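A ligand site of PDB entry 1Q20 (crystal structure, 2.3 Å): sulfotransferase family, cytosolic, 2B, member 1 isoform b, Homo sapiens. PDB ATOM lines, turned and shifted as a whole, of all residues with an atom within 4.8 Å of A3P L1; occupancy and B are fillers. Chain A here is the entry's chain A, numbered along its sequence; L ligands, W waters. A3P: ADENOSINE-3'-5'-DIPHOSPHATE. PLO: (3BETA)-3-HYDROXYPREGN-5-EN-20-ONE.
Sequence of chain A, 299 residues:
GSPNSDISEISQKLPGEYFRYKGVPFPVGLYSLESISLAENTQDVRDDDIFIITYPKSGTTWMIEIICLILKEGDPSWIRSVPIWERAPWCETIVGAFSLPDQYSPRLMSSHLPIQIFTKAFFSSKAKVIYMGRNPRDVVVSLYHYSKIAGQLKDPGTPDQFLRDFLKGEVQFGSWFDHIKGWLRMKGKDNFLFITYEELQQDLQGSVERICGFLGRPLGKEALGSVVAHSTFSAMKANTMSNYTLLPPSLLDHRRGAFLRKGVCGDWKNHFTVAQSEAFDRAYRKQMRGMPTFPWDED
NE1 of Trp 62 lies close to N6 of A3P L1. Residues that only touch A3P L1: Leu 260 (3.4 Å), Phe 259 (3.4 Å), Phe 233 (3.4 Å) and Thr 232 (3.8 Å). Hydrophobic or aromatic side chains that line A3P L1: Trp 62, Tyr 197, Phe 233, Met 236, Phe 259 and Leu 260. Within 4 Å of A3P L1: Lys 57, Ser 58, Gly 59, Thr 60, Thr 61, Trp 62, Arg 134, Ser 142, Tyr 197, Ser 231, Thr 232, Phe 233, Met 236, Phe 259, Leu 260, Arg 261, Lys 262 and Gly 263. Along chain A the residues within 4 Å of A3P L1 span positions 57 to 263.
O1P of A3P L1 lies within salt-bridge range of NE of Arg 261, 3.0 Å away. The backbone NH of Thr 61 is in hydrogen-bond range of an oxygen (O5P) of A3P L1, 2.9 Å away. A ring nitrogen (NE2) of His 112 sits at hydrogen-bond distance from an oxygen (O3) of PLO L2 (2.7 Å). The backbone NH (N) of Gly 263 sits at hydrogen-bond distance from an oxygen (O2P) of A3P L1. N6 of A3P L1 is in hydrogen-bond range of O of Ser 231. N of Thr 60 lies within hydrogen-bond range of O4P of A3P L1, at 2.8 Å. NZ of Lys 57 is in salt-bridge range of O6P of A3P L1 (3.0 Å). The side-chain hydroxyl of Tyr 197 lies within hydrogen-bond range of a nitrogen (N3) of A3P L1 (2.8 Å). The backbone NH (N) of Gly 59 is in hydrogen-bond range of an oxygen (O4P) of A3P L1. N of Lys 262 lies within hydrogen-bond range of O2P of A3P L1 (2.8 Å). N of Lys 57 sits at hydrogen-bond distance from O4P of A3P L1, 3.3 Å away. The side-chain hydroxyl (OG1) of Thr 60 is in hydrogen-bond range of an oxygen (O4P) of A3P L1, at 2.5 Å. The side-chain hydroxyl (OG1) of Thr 61 is in hydrogen-bond range of an oxygen (O5P) of A3P L1 (2.8 Å). OG of Ser 142 lies within hydrogen-bond range of O1P of A3P L1 (2.8 Å). SD of Met 236 lies within hydrogen-bond range of N6 of A3P L1, 3.2 Å away. The backbone NH (N) of Ser 58 lies within hydrogen-bond range of an oxygen (O4P) of A3P L1. An oxygen (O3P) of A3P L1 is in salt-bridge range of the guanidinium group of Arg 134.
The side-chain hydroxyl of Thr 54 is in hydrogen-bond range of the side-chain hydroxyl of Thr 60, at 2.7 Å. The backbone carbonyl oxygen (O) of Lys 57 sits at hydrogen-bond distance from the guanidinium group (NH1) of Arg 134, 3.2 Å away. N of Val 264 lies within hydrogen-bond range of OH of Tyr 197. OG of Ser 58 sits at hydrogen-bond distance from O of Tyr 55 (2.6 Å). The side-chain hydroxyl (OH) of Tyr 197 is in hydrogen-bond range of the side-chain amide nitrogen (NE2) of Gln 201, 3.1 Å away. The backbone carbonyl oxygen of Gly 263 lies within hydrogen-bond range of the side-chain amide nitrogen of Gln 201. The side-chain hydroxyl (OH) of Tyr 197 lies close to the backbone carbonyl oxygen (O) of Gly 263, 3.3 Å away. O of Ser 231 lies within hydrogen-bond range of NE1 of Trp 62.
Water W4 bridges a nitrogen (N1) of A3P L1 (2.7 Å) and the backbone NH (N) of Phe 233 (2.9 Å). Water W3 lies within hydrogen-bond range of O6P of A3P L1 (2.8 Å) and O3 of PLO L2 (2.9 Å). Water W1 lies within hydrogen-bond range of an oxygen (O3P) of A3P L1 (2.8 Å), the backbone NH of Val 264 (2.9 Å) and the backbone NH of Gly 263 (3.3 Å). Water W2 lies within hydrogen-bond range of O1P of A3P L1 (2.8 Å) and O of Ser 142 (2.9 Å). Water W5 lies within hydrogen-bond range of O3P of A3P L1 (2.9 Å), NH2 of Arg 261 (3.3 Å) and NH2 of Arg 134 (3.4 Å).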
ATOM      1  N   THR A  54     -21.713 -17.440   1.247  1.00  0.00           N
ATOM      2  CA  THR A  54     -21.125 -16.818   2.429  1.00  0.00           C
ATOM      3  C   THR A  54     -21.977 -15.689   2.980  1.00  0.00           C
ATOM      4  O   THR A  54     -22.877 -15.176   2.315  1.00  0.00           O
ATOM      5  CB  THR A  54     -19.767 -16.158   2.090  1.00  0.00           C
ATOM      6  OG1 THR A  54     -19.992 -15.099   1.140  1.00  0.00           O
ATOM      7  CG2 THR A  54     -18.788 -17.159   1.538  1.00  0.00           C
ATOM      8  N   TYR A  55     -21.694 -15.319   4.219  1.00  0.00           N
ATOM      9  CA  TYR A  55     -22.344 -14.176   4.820  1.00  0.00           C
ATOM     10  C   TYR A  55     -21.340 -13.099   4.341  1.00  0.00           C
ATOM     11  O   TYR A  55     -20.138 -13.329   4.382  1.00  0.00           O
ATOM     12  CB  TYR A  55     -22.326 -14.254   6.352  1.00  0.00           C
ATOM     13  CG  TYR A  55     -23.041 -13.081   6.997  1.00  0.00           C
ATOM     14  CD1 TYR A  55     -24.426 -13.021   7.015  1.00  0.00           C
ATOM     15  CD2 TYR A  55     -22.316 -12.005   7.527  1.00  0.00           C
ATOM     16  CE1 TYR A  55     -25.087 -11.919   7.547  1.00  0.00           C
ATOM     17  CE2 TYR A  55     -22.970 -10.897   8.053  1.00  0.00           C
ATOM     18  CZ  TYR A  55     -24.361 -10.859   8.062  1.00  0.00           C
ATOM     19  OH  TYR A  55     -25.018  -9.761   8.558  1.00  0.00           O
ATOM     20  N   PRO A  56     -21.826 -11.935   3.890  1.00  0.00           N
ATOM     21  CA  PRO A  56     -20.915 -10.879   3.409  1.00  0.00           C
ATOM     22  C   PRO A  56     -19.667 -10.625   4.270  1.00  0.00           C
ATOM     23  O   PRO A  56     -19.731 -10.648   5.506  1.00  0.00           O
ATOM     24  CB  PRO A  56     -21.823  -9.655   3.337  1.00  0.00           C
ATOM     25  CG  PRO A  56     -23.159 -10.283   2.939  1.00  0.00           C
ATOM     26  CD  PRO A  56     -23.227 -11.484   3.864  1.00  0.00           C
ATOM     27  N   LYS A  57     -18.547 -10.405   3.597  1.00  0.00           N
ATOM     28  CA  LYS A  57     -17.231 -10.126   4.199  1.00  0.00           C
ATOM     29  C   LYS A  57     -16.566 -11.298   4.904  1.00  0.00           C
ATOM     30  O   LYS A  57     -15.752 -11.100   5.802  1.00  0.00           O
ATOM     31  CB  LYS A  57     -17.313  -8.957   5.195  1.00  0.00           C
ATOM     32  CG  LYS A  57     -18.232  -7.820   4.776  1.00  0.00           C
ATOM     33  CD  LYS A  57     -18.118  -7.501   3.284  1.00  0.00           C
ATOM     34  CE  LYS A  57     -16.719  -7.012   2.884  1.00  0.00           C
ATOM     35  NZ  LYS A  57     -16.667  -6.708   1.412  1.00  0.00           N
ATOM     36  N   SER A  58     -16.891 -12.521   4.483  1.00  0.00           N
ATOM     37  CA  SER A  58     -16.288 -13.701   5.108  1.00  0.00           C
ATOM     38  C   SER A  58     -15.122 -14.257   4.293  1.00  0.00           C
ATOM     39  O   SER A  58     -14.513 -15.270   4.669  1.00  0.00           O
ATOM     40  CB  SER A  58     -17.342 -14.794   5.298  1.00  0.00           C
ATOM     41  OG  SER A  58     -18.448 -14.295   6.038  1.00  0.00           O
ATOM     42  N   GLY A  59     -14.796 -13.584   3.183  1.00  0.00           N
ATOM     43  CA  GLY A  59     -13.700 -14.016   2.333  1.00  0.00           C
ATOM     44  C   GLY A  59     -14.169 -14.683   1.048  1.00  0.00           C
ATOM     45  O   GLY A  59     -13.502 -15.564   0.516  1.00  0.00           O
ATOM     46  N   THR A  60     -15.326 -14.249   0.550  1.00  0.00           N
ATOM     47  CA  THR A  60     -15.902 -14.782  -0.678  1.00  0.00           C
ATOM     48  C   THR A  60     -14.916 -14.646  -1.838  1.00  0.00           C
ATOM     49  O   THR A  60     -14.658 -15.599  -2.588  1.00  0.00           O
ATOM     50  CB  THR A  60     -17.180 -14.011  -1.051  1.00  0.00           C
ATOM     51  OG1 THR A  60     -17.943 -13.730   0.132  1.00  0.00           O
ATOM     52  CG2 THR A  60     -18.023 -14.818  -2.039  1.00  0.00           C
ATOM     53  N   THR A  61     -14.364 -13.443  -1.966  1.00  0.00           N
ATOM     54  CA  THR A  61     -13.410 -13.128  -3.012  1.00  0.00           C
ATOM     55  C   THR A  61     -12.285 -14.146  -2.997  1.00  0.00           C
ATOM     56  O   THR A  61     -11.857 -14.620  -4.049  1.00  0.00           O
ATOM     57  CB  THR A  61     -12.793 -11.729  -2.805  1.00  0.00           C
ATOM     58  OG1 THR A  61     -13.826 -10.750  -2.696  1.00  0.00           O
ATOM     59  CG2 THR A  61     -11.881 -11.371  -3.984  1.00  0.00           C
ATOM     60  N   TRP A  62     -11.810 -14.485  -1.812  1.00  0.00           N
ATOM     61  CA  TRP A  62     -10.728 -15.451  -1.690  1.00  0.00           C
ATOM     62  C   TRP A  62     -11.130 -16.784  -2.322  1.00  0.00           C
ATOM     63  O   TRP A  62     -10.481 -17.268  -3.255  1.00  0.00           O
ATOM     64  CB  TRP A  62     -10.395 -15.641  -0.222  1.00  0.00           C
ATOM     65  CG  TRP A  62      -9.023 -16.197   0.049  1.00  0.00           C
ATOM     66  CD1 TRP A  62      -8.116 -16.637  -0.884  1.00  0.00           C
ATOM     67  CD2 TRP A  62      -8.388 -16.325   1.330  1.00  0.00           C
ATOM     68  NE1 TRP A  62      -6.942 -17.024  -0.250  1.00  0.00           N
ATOM     69  CE2 TRP A  62      -7.094 -16.838   1.102  1.00  0.00           C
ATOM     70  CE3 TRP A  62      -8.795 -16.046   2.637  1.00  0.00           C
ATOM     71  CZ2 TRP A  62      -6.189 -17.077   2.141  1.00  0.00           C
ATOM     72  CZ3 TRP A  62      -7.893 -16.286   3.690  1.00  0.00           C
ATOM     73  CH2 TRP A  62      -6.609 -16.801   3.430  1.00  0.00           C
ATOM     74  N   HIS A 112     -24.982 -14.739  -1.352  1.00  0.00           N
ATOM     75  CA  HIS A 112     -24.957 -14.361   0.063  1.00  0.00           C
ATOM     76  C   HIS A 112     -26.325 -14.698   0.679  1.00  0.00           C
ATOM     77  O   HIS A 112     -26.586 -14.378   1.833  1.00  0.00           O
ATOM     78  CB  HIS A 112     -24.712 -12.857   0.225  1.00  0.00           C
ATOM     79  CG  HIS A 112     -23.310 -12.429  -0.066  1.00  0.00           C
ATOM     80  ND1 HIS A 112     -22.206 -13.127   0.390  1.00  0.00           N
ATOM     81  CD2 HIS A 112     -22.820 -11.347  -0.723  1.00  0.00           C
ATOM     82  CE1 HIS A 112     -21.104 -12.498   0.030  1.00  0.00           C
ATOM     83  NE2 HIS A 112     -21.448 -11.416  -0.657  1.00  0.00           N
ATOM     84  N   ARG A 134     -16.489 -17.045   8.729  1.00  0.00           N
ATOM     85  CA  ARG A 134     -15.363 -16.292   9.289  1.00  0.00           C
ATOM     86  C   ARG A 134     -15.738 -15.789  10.683  1.00  0.00           C
ATOM     87  O   ARG A 134     -16.917 -15.673  10.994  1.00  0.00           O
ATOM     88  CB  ARG A 134     -15.039 -15.083   8.399  1.00  0.00           C
ATOM     89  CG  ARG A 134     -13.795 -14.277   8.786  1.00  0.00           C
ATOM     90  CD  ARG A 134     -13.616 -13.037   7.919  1.00  0.00           C
ATOM     91  NE  ARG A 134     -12.324 -12.392   8.139  1.00  0.00           N
ATOM     92  CZ  ARG A 134     -11.951 -11.247   7.586  1.00  0.00           C
ATOM     93  NH1 ARG A 134     -12.767 -10.596   6.770  1.00  0.00           N
ATOM     94  NH2 ARG A 134     -10.745 -10.754   7.831  1.00  0.00           N
ATOM     95  N   SER A 142     -14.707  -5.724   9.018  1.00  0.00           N
ATOM     96  CA  SER A 142     -14.569  -5.674   7.568  1.00  0.00           C
ATOM     97  C   SER A 142     -15.764  -5.008   6.921  1.00  0.00           C
ATOM     98  O   SER A 142     -15.643  -4.212   5.998  1.00  0.00           O
ATOM     99  CB  SER A 142     -14.403  -7.094   7.007  1.00  0.00           C
ATOM    100  OG  SER A 142     -14.424  -7.094   5.596  1.00  0.00           O
ATOM    101  N   TYR A 197     -12.524 -19.033   6.864  1.00  0.00           N
ATOM    102  CA  TYR A 197     -11.513 -18.047   6.522  1.00  0.00           C
ATOM    103  C   TYR A 197     -10.264 -18.346   7.345  1.00  0.00           C
ATOM    104  O   TYR A 197      -9.137 -18.209   6.854  1.00  0.00           O
ATOM    105  CB  TYR A 197     -12.051 -16.659   6.874  1.00  0.00           C
ATOM    106  CG  TYR A 197     -11.105 -15.514   6.571  1.00  0.00           C
ATOM    107  CD1 TYR A 197     -11.079 -14.916   5.313  1.00  0.00           C
ATOM    108  CD2 TYR A 197     -10.225 -15.032   7.545  1.00  0.00           C
ATOM    109  CE1 TYR A 197     -10.205 -13.868   5.033  1.00  0.00           C
ATOM    110  CE2 TYR A 197      -9.348 -13.991   7.281  1.00  0.00           C
ATOM    111  CZ  TYR A 197      -9.341 -13.414   6.017  1.00  0.00           C
ATOM    112  OH  TYR A 197      -8.465 -12.406   5.737  1.00  0.00           O
ATOM    113  N   GLN A 201      -6.294 -19.302   6.233  1.00  0.00           N
ATOM    114  CA  GLN A 201      -5.201 -18.501   6.766  1.00  0.00           C
ATOM    115  C   GLN A 201      -4.149 -19.376   7.444  1.00  0.00           C
ATOM    116  O   GLN A 201      -2.952 -19.089   7.375  1.00  0.00           O
ATOM    117  CB  GLN A 201      -5.733 -17.470   7.757  1.00  0.00           C
ATOM    118  CG  GLN A 201      -6.420 -16.281   7.098  1.00  0.00           C
ATOM    119  CD  GLN A 201      -5.437 -15.194   6.693  1.00  0.00           C
ATOM    120  OE1 GLN A 201      -4.255 -15.462   6.459  1.00  0.00           O
ATOM    121  NE2 GLN A 201      -5.925 -13.958   6.579  1.00  0.00           N
ATOM    122  N   SER A 231      -3.498 -17.075  -5.042  1.00  0.00           N
ATOM    123  CA  SER A 231      -4.615 -16.903  -4.103  1.00  0.00           C
ATOM    124  C   SER A 231      -4.224 -16.073  -2.897  1.00  0.00           C
ATOM    125  O   SER A 231      -5.075 -15.667  -2.112  1.00  0.00           O
ATOM    126  CB  SER A 231      -5.104 -18.257  -3.577  1.00  0.00           C
ATOM    127  OG  SER A 231      -5.778 -18.996  -4.573  1.00  0.00           O
ATOM    128  N   THR A 232      -2.928 -15.839  -2.739  1.00  0.00           N
ATOM    129  CA  THR A 232      -2.426 -15.085  -1.603  1.00  0.00           C
ATOM    130  C   THR A 232      -2.957 -13.669  -1.613  1.00  0.00           C
ATOM    131  O   THR A 232      -3.217 -13.101  -2.673  1.00  0.00           O
ATOM    132  CB  THR A 232      -0.893 -15.121  -1.606  1.00  0.00           C
ATOM    133  OG1 THR A 232      -0.465 -16.486  -1.613  1.00  0.00           O
ATOM    134  CG2 THR A 232      -0.339 -14.480  -0.373  1.00  0.00           C
ATOM    135  N   PHE A 233      -3.141 -13.092  -0.433  1.00  0.00           N
ATOM    136  CA  PHE A 233      -3.655 -11.745  -0.309  1.00  0.00           C
ATOM    137  C   PHE A 233      -2.860 -10.742  -1.156  1.00  0.00           C
ATOM    138  O   PHE A 233      -3.458  -9.980  -1.937  1.00  0.00           O
ATOM    139  CB  PHE A 233      -3.630 -11.300   1.152  1.00  0.00           C
ATOM    140  CG  PHE A 233      -4.199  -9.928   1.379  1.00  0.00           C
ATOM    141  CD1 PHE A 233      -5.568  -9.708   1.333  1.00  0.00           C
ATOM    142  CD2 PHE A 233      -3.350  -8.842   1.576  1.00  0.00           C
ATOM    143  CE1 PHE A 233      -6.089  -8.432   1.489  1.00  0.00           C
ATOM    144  CE2 PHE A 233      -3.867  -7.561   1.740  1.00  0.00           C
ATOM    145  CZ  PHE A 233      -5.239  -7.359   1.693  1.00  0.00           C
ATOM    146  N   MET A 236      -3.487 -11.226  -4.937  1.00  0.00           N
ATOM    147  CA  MET A 236      -4.834 -10.813  -5.315  1.00  0.00           C
ATOM    148  C   MET A 236      -5.029  -9.306  -5.210  1.00  0.00           C
ATOM    149  O   MET A 236      -5.786  -8.714  -5.977  1.00  0.00           O
ATOM    150  CB  MET A 236      -5.870 -11.537  -4.447  1.00  0.00           C
ATOM    151  CG  MET A 236      -6.052 -13.014  -4.782  1.00  0.00           C
ATOM    152  SD  MET A 236      -7.366 -13.805  -3.795  1.00  0.00           S
ATOM    153  CE  MET A 236      -8.802 -12.922  -4.370  1.00  0.00           C
ATOM    154  N   PHE A 259     -11.204  -2.806  -1.429  1.00  0.00           N
ATOM    155  CA  PHE A 259     -12.026  -3.965  -1.104  1.00  0.00           C
ATOM    156  C   PHE A 259     -11.154  -4.933  -0.291  1.00  0.00           C
ATOM    157  O   PHE A 259     -11.576  -5.464   0.734  1.00  0.00           O
ATOM    158  CB  PHE A 259     -12.504  -4.642  -2.392  1.00  0.00           C
ATOM    159  CG  PHE A 259     -13.612  -5.669  -2.184  1.00  0.00           C
ATOM    160  CD1 PHE A 259     -14.931  -5.358  -2.500  1.00  0.00           C
ATOM    161  CD2 PHE A 259     -13.322  -6.936  -1.698  1.00  0.00           C
ATOM    162  CE1 PHE A 259     -15.936  -6.309  -2.352  1.00  0.00           C
ATOM    163  CE2 PHE A 259     -14.330  -7.887  -1.536  1.00  0.00           C
ATOM    164  CZ  PHE A 259     -15.639  -7.582  -1.864  1.00  0.00           C
ATOM    165  N   LEU A 260      -9.929  -5.168  -0.768  1.00  0.00           N
ATOM    166  CA  LEU A 260      -9.008  -6.033  -0.035  1.00  0.00           C
ATOM    167  C   LEU A 260      -8.254  -5.110   0.906  1.00  0.00           C
ATOM    168  O   LEU A 260      -7.154  -4.643   0.607  1.00  0.00           O
ATOM    169  CB  LEU A 260      -8.035  -6.739  -0.981  1.00  0.00           C
ATOM    170  CG  LEU A 260      -8.626  -7.642  -2.056  1.00  0.00           C
ATOM    171  CD1 LEU A 260      -7.510  -8.490  -2.665  1.00  0.00           C
ATOM    172  CD2 LEU A 260      -9.679  -8.544  -1.466  1.00  0.00           C
ATOM    173  N   ARG A 261      -8.906  -4.843   2.043  1.00  0.00           N
ATOM    174  CA  ARG A 261      -8.434  -3.951   3.095  1.00  0.00           C
ATOM    175  C   ARG A 261      -7.173  -4.411   3.851  1.00  0.00           C
ATOM    176  O   ARG A 261      -6.122  -3.788   3.698  1.00  0.00           O
ATOM    177  CB  ARG A 261      -9.594  -3.728   4.069  1.00  0.00           C
ATOM    178  CG  ARG A 261      -9.399  -2.623   5.074  1.00  0.00           C
ATOM    179  CD  ARG A 261     -10.628  -2.560   5.961  1.00  0.00           C
ATOM    180  NE  ARG A 261     -10.791  -3.790   6.730  1.00  0.00           N
ATOM    181  CZ  ARG A 261     -10.166  -4.030   7.875  1.00  0.00           C
ATOM    182  NH1 ARG A 261      -9.350  -3.112   8.379  1.00  0.00           N
ATOM    183  NH2 ARG A 261     -10.356  -5.173   8.517  1.00  0.00           N
ATOM    184  N   LYS A 262      -7.271  -5.466   4.663  1.00  0.00           N
ATOM    185  CA  LYS A 262      -6.112  -5.958   5.415  1.00  0.00           C
ATOM    186  C   LYS A 262      -5.821  -7.440   5.175  1.00  0.00           C
ATOM    187  O   LYS A 262      -4.656  -7.830   5.057  1.00  0.00           O
ATOM    188  CB  LYS A 262      -6.283  -5.743   6.917  1.00  0.00           C
ATOM    189  CG  LYS A 262      -5.909  -4.373   7.390  1.00  0.00           C
ATOM    190  CD  LYS A 262      -5.812  -4.303   8.902  1.00  0.00           C
ATOM    191  CE  LYS A 262      -4.692  -5.189   9.415  1.00  0.00           C
ATOM    192  NZ  LYS A 262      -4.303  -4.821  10.810  1.00  0.00           N
ATOM    193  N   GLY A 263      -6.862  -8.252   5.143  1.00  0.00           N
ATOM    194  CA  GLY A 263      -6.674  -9.666   4.901  1.00  0.00           C
ATOM    195  C   GLY A 263      -6.040 -10.513   5.987  1.00  0.00           C
ATOM    196  O   GLY A 263      -5.275 -11.434   5.675  1.00  0.00           O
ATOM    197  N   VAL A 264      -6.320 -10.215   7.260  1.00  0.00           N
ATOM    198  CA  VAL A 264      -5.779 -11.008   8.361  1.00  0.00           C
ATOM    199  C   VAL A 264      -6.915 -11.463   9.278  1.00  0.00           C
ATOM    200  O   VAL A 264      -8.084 -11.155   9.043  1.00  0.00           O
ATOM    201  CB  VAL A 264      -4.770 -10.217   9.237  1.00  0.00           C
ATOM    202  CG1 VAL A 264      -3.567  -9.777   8.402  1.00  0.00           C
ATOM    203  CG2 VAL A 264      -5.460  -9.010   9.852  1.00  0.00           C
HETATM  204  P1  A3P L   1     -10.809  -7.421   5.514  1.00  0.00           P
HETATM  205  O1P A3P L   1     -11.782  -6.290   5.314  1.00  0.00           O
HETATM  206  O2P A3P L   1      -9.485  -7.086   4.954  1.00  0.00           O
HETATM  207  O3P A3P L   1     -10.699  -7.820   6.921  1.00  0.00           O
HETATM  208  P2  A3P L   1     -15.834 -10.827   0.938  1.00  0.00           P
HETATM  209  O4P A3P L   1     -16.689 -11.943   1.410  1.00  0.00           O
HETATM  210  O5P A3P L   1     -15.122 -11.225  -0.289  1.00  0.00           O
HETATM  211  O6P A3P L   1     -16.621  -9.604   0.699  1.00  0.00           O
HETATM  212  O5' A3P L   1     -14.762 -10.530   2.085  1.00  0.00           O
HETATM  213  C5' A3P L   1     -13.729  -9.557   1.973  1.00  0.00           C
HETATM  214  C4' A3P L   1     -12.714  -9.799   3.083  1.00  0.00           C
HETATM  215  O4' A3P L   1     -11.904 -10.962   2.703  1.00  0.00           O
HETATM  216  C3' A3P L   1     -11.723  -8.666   3.309  1.00  0.00           C
HETATM  217  O3' A3P L   1     -11.371  -8.679   4.713  1.00  0.00           O
HETATM  218  C2' A3P L   1     -10.594  -9.068   2.380  1.00  0.00           C
HETATM  219  O2' A3P L   1      -9.348  -8.436   2.552  1.00  0.00           O
HETATM  220  C1' A3P L   1     -10.534 -10.581   2.672  1.00  0.00           C
HETATM  221  N9  A3P L   1      -9.793 -11.299   1.624  1.00  0.00           N
HETATM  222  C8  A3P L   1     -10.076 -11.393   0.270  1.00  0.00           C
HETATM  223  N7  A3P L   1      -9.207 -12.101  -0.404  1.00  0.00           N
HETATM  224  C5  A3P L   1      -8.290 -12.506   0.546  1.00  0.00           C
HETATM  225  C6  A3P L   1      -7.120 -13.280   0.484  1.00  0.00           C
HETATM  226  N6  A3P L   1      -6.655 -13.807  -0.648  1.00  0.00           N
HETATM  227  N1  A3P L   1      -6.423 -13.515   1.647  1.00  0.00           N
HETATM  228  C2  A3P L   1      -6.878 -12.986   2.811  1.00  0.00           C
HETATM  229  N3  A3P L   1      -7.981 -12.218   2.998  1.00  0.00           N
HETATM  230  C4  A3P L   1      -8.643 -12.023   1.821  1.00  0.00           C
HETATM  231  C1  PLO L   2     -22.406  -7.965  -4.691  1.00  0.00           C
HETATM  232  C2  PLO L   2     -21.970  -8.460  -3.250  1.00  0.00           C
HETATM  233  C3  PLO L   2     -20.495  -8.942  -3.185  1.00  0.00           C
HETATM  234  O3  PLO L   2     -20.091  -9.391  -1.846  1.00  0.00           O
HETATM  235  C4  PLO L   2     -19.476  -7.837  -3.675  1.00  0.00           C
HETATM  236  C5  PLO L   2     -19.839  -7.319  -5.083  1.00  0.00           C
HETATM  237  C6  PLO L   2     -18.751  -7.087  -6.141  1.00  0.00           C
HETATM  238  C7  PLO L   2     -19.055  -6.555  -7.556  1.00  0.00           C
HETATM  239  C8  PLO L   2     -20.580  -6.199  -7.906  1.00  0.00           C
HETATM  240  C9  PLO L   2     -21.583  -7.109  -7.123  1.00  0.00           C
HETATM  241  C10 PLO L   2     -21.383  -6.970  -5.569  1.00  0.00           C
HETATM  242  C11 PLO L   2     -23.046  -6.785  -7.503  1.00  0.00           C
HETATM  243  C12 PLO L   2     -23.291  -6.891  -9.023  1.00  0.00           C
HETATM  244  C13 PLO L   2     -22.332  -5.960  -9.838  1.00  0.00           C
HETATM  245  C14 PLO L   2     -20.852  -6.360  -9.420  1.00  0.00           C
HETATM  246  C15 PLO L   2     -20.013  -5.568 -10.451  1.00  0.00           C
HETATM  247  C16 PLO L   2     -20.771  -5.771 -11.758  1.00  0.00           C
HETATM  248  C17 PLO L   2     -22.236  -6.219 -11.396  1.00  0.00           C
HETATM  249  C18 PLO L   2     -22.661  -4.459  -9.534  1.00  0.00           C
HETATM  250  C19 PLO L   2     -21.768  -5.578  -4.983  1.00  0.00           C
HETATM  251  C20 PLO L   2     -23.288  -5.455 -12.252  1.00  0.00           C
HETATM  252  C21 PLO L   2     -24.711  -5.899 -12.127  1.00  0.00           C
HETATM  253  O20 PLO L   2     -23.006  -4.535 -13.016  1.00  0.00           O
HETATM  254  O   HOH W   1      -8.206  -8.140   8.159  1.00  0.00           O
HETATM  255  O   HOH W   2     -13.439  -4.333   4.169  1.00  0.00           O
HETATM  256  O   HOH W   3     -17.519 -10.663  -1.708  1.00  0.00           O
HETATM  257  O   HOH W   4      -4.042 -14.705   1.856  1.00  0.00           O
HETATM  258  O   HOH W   5     -11.717  -7.993   9.631  1.00  0.00           O
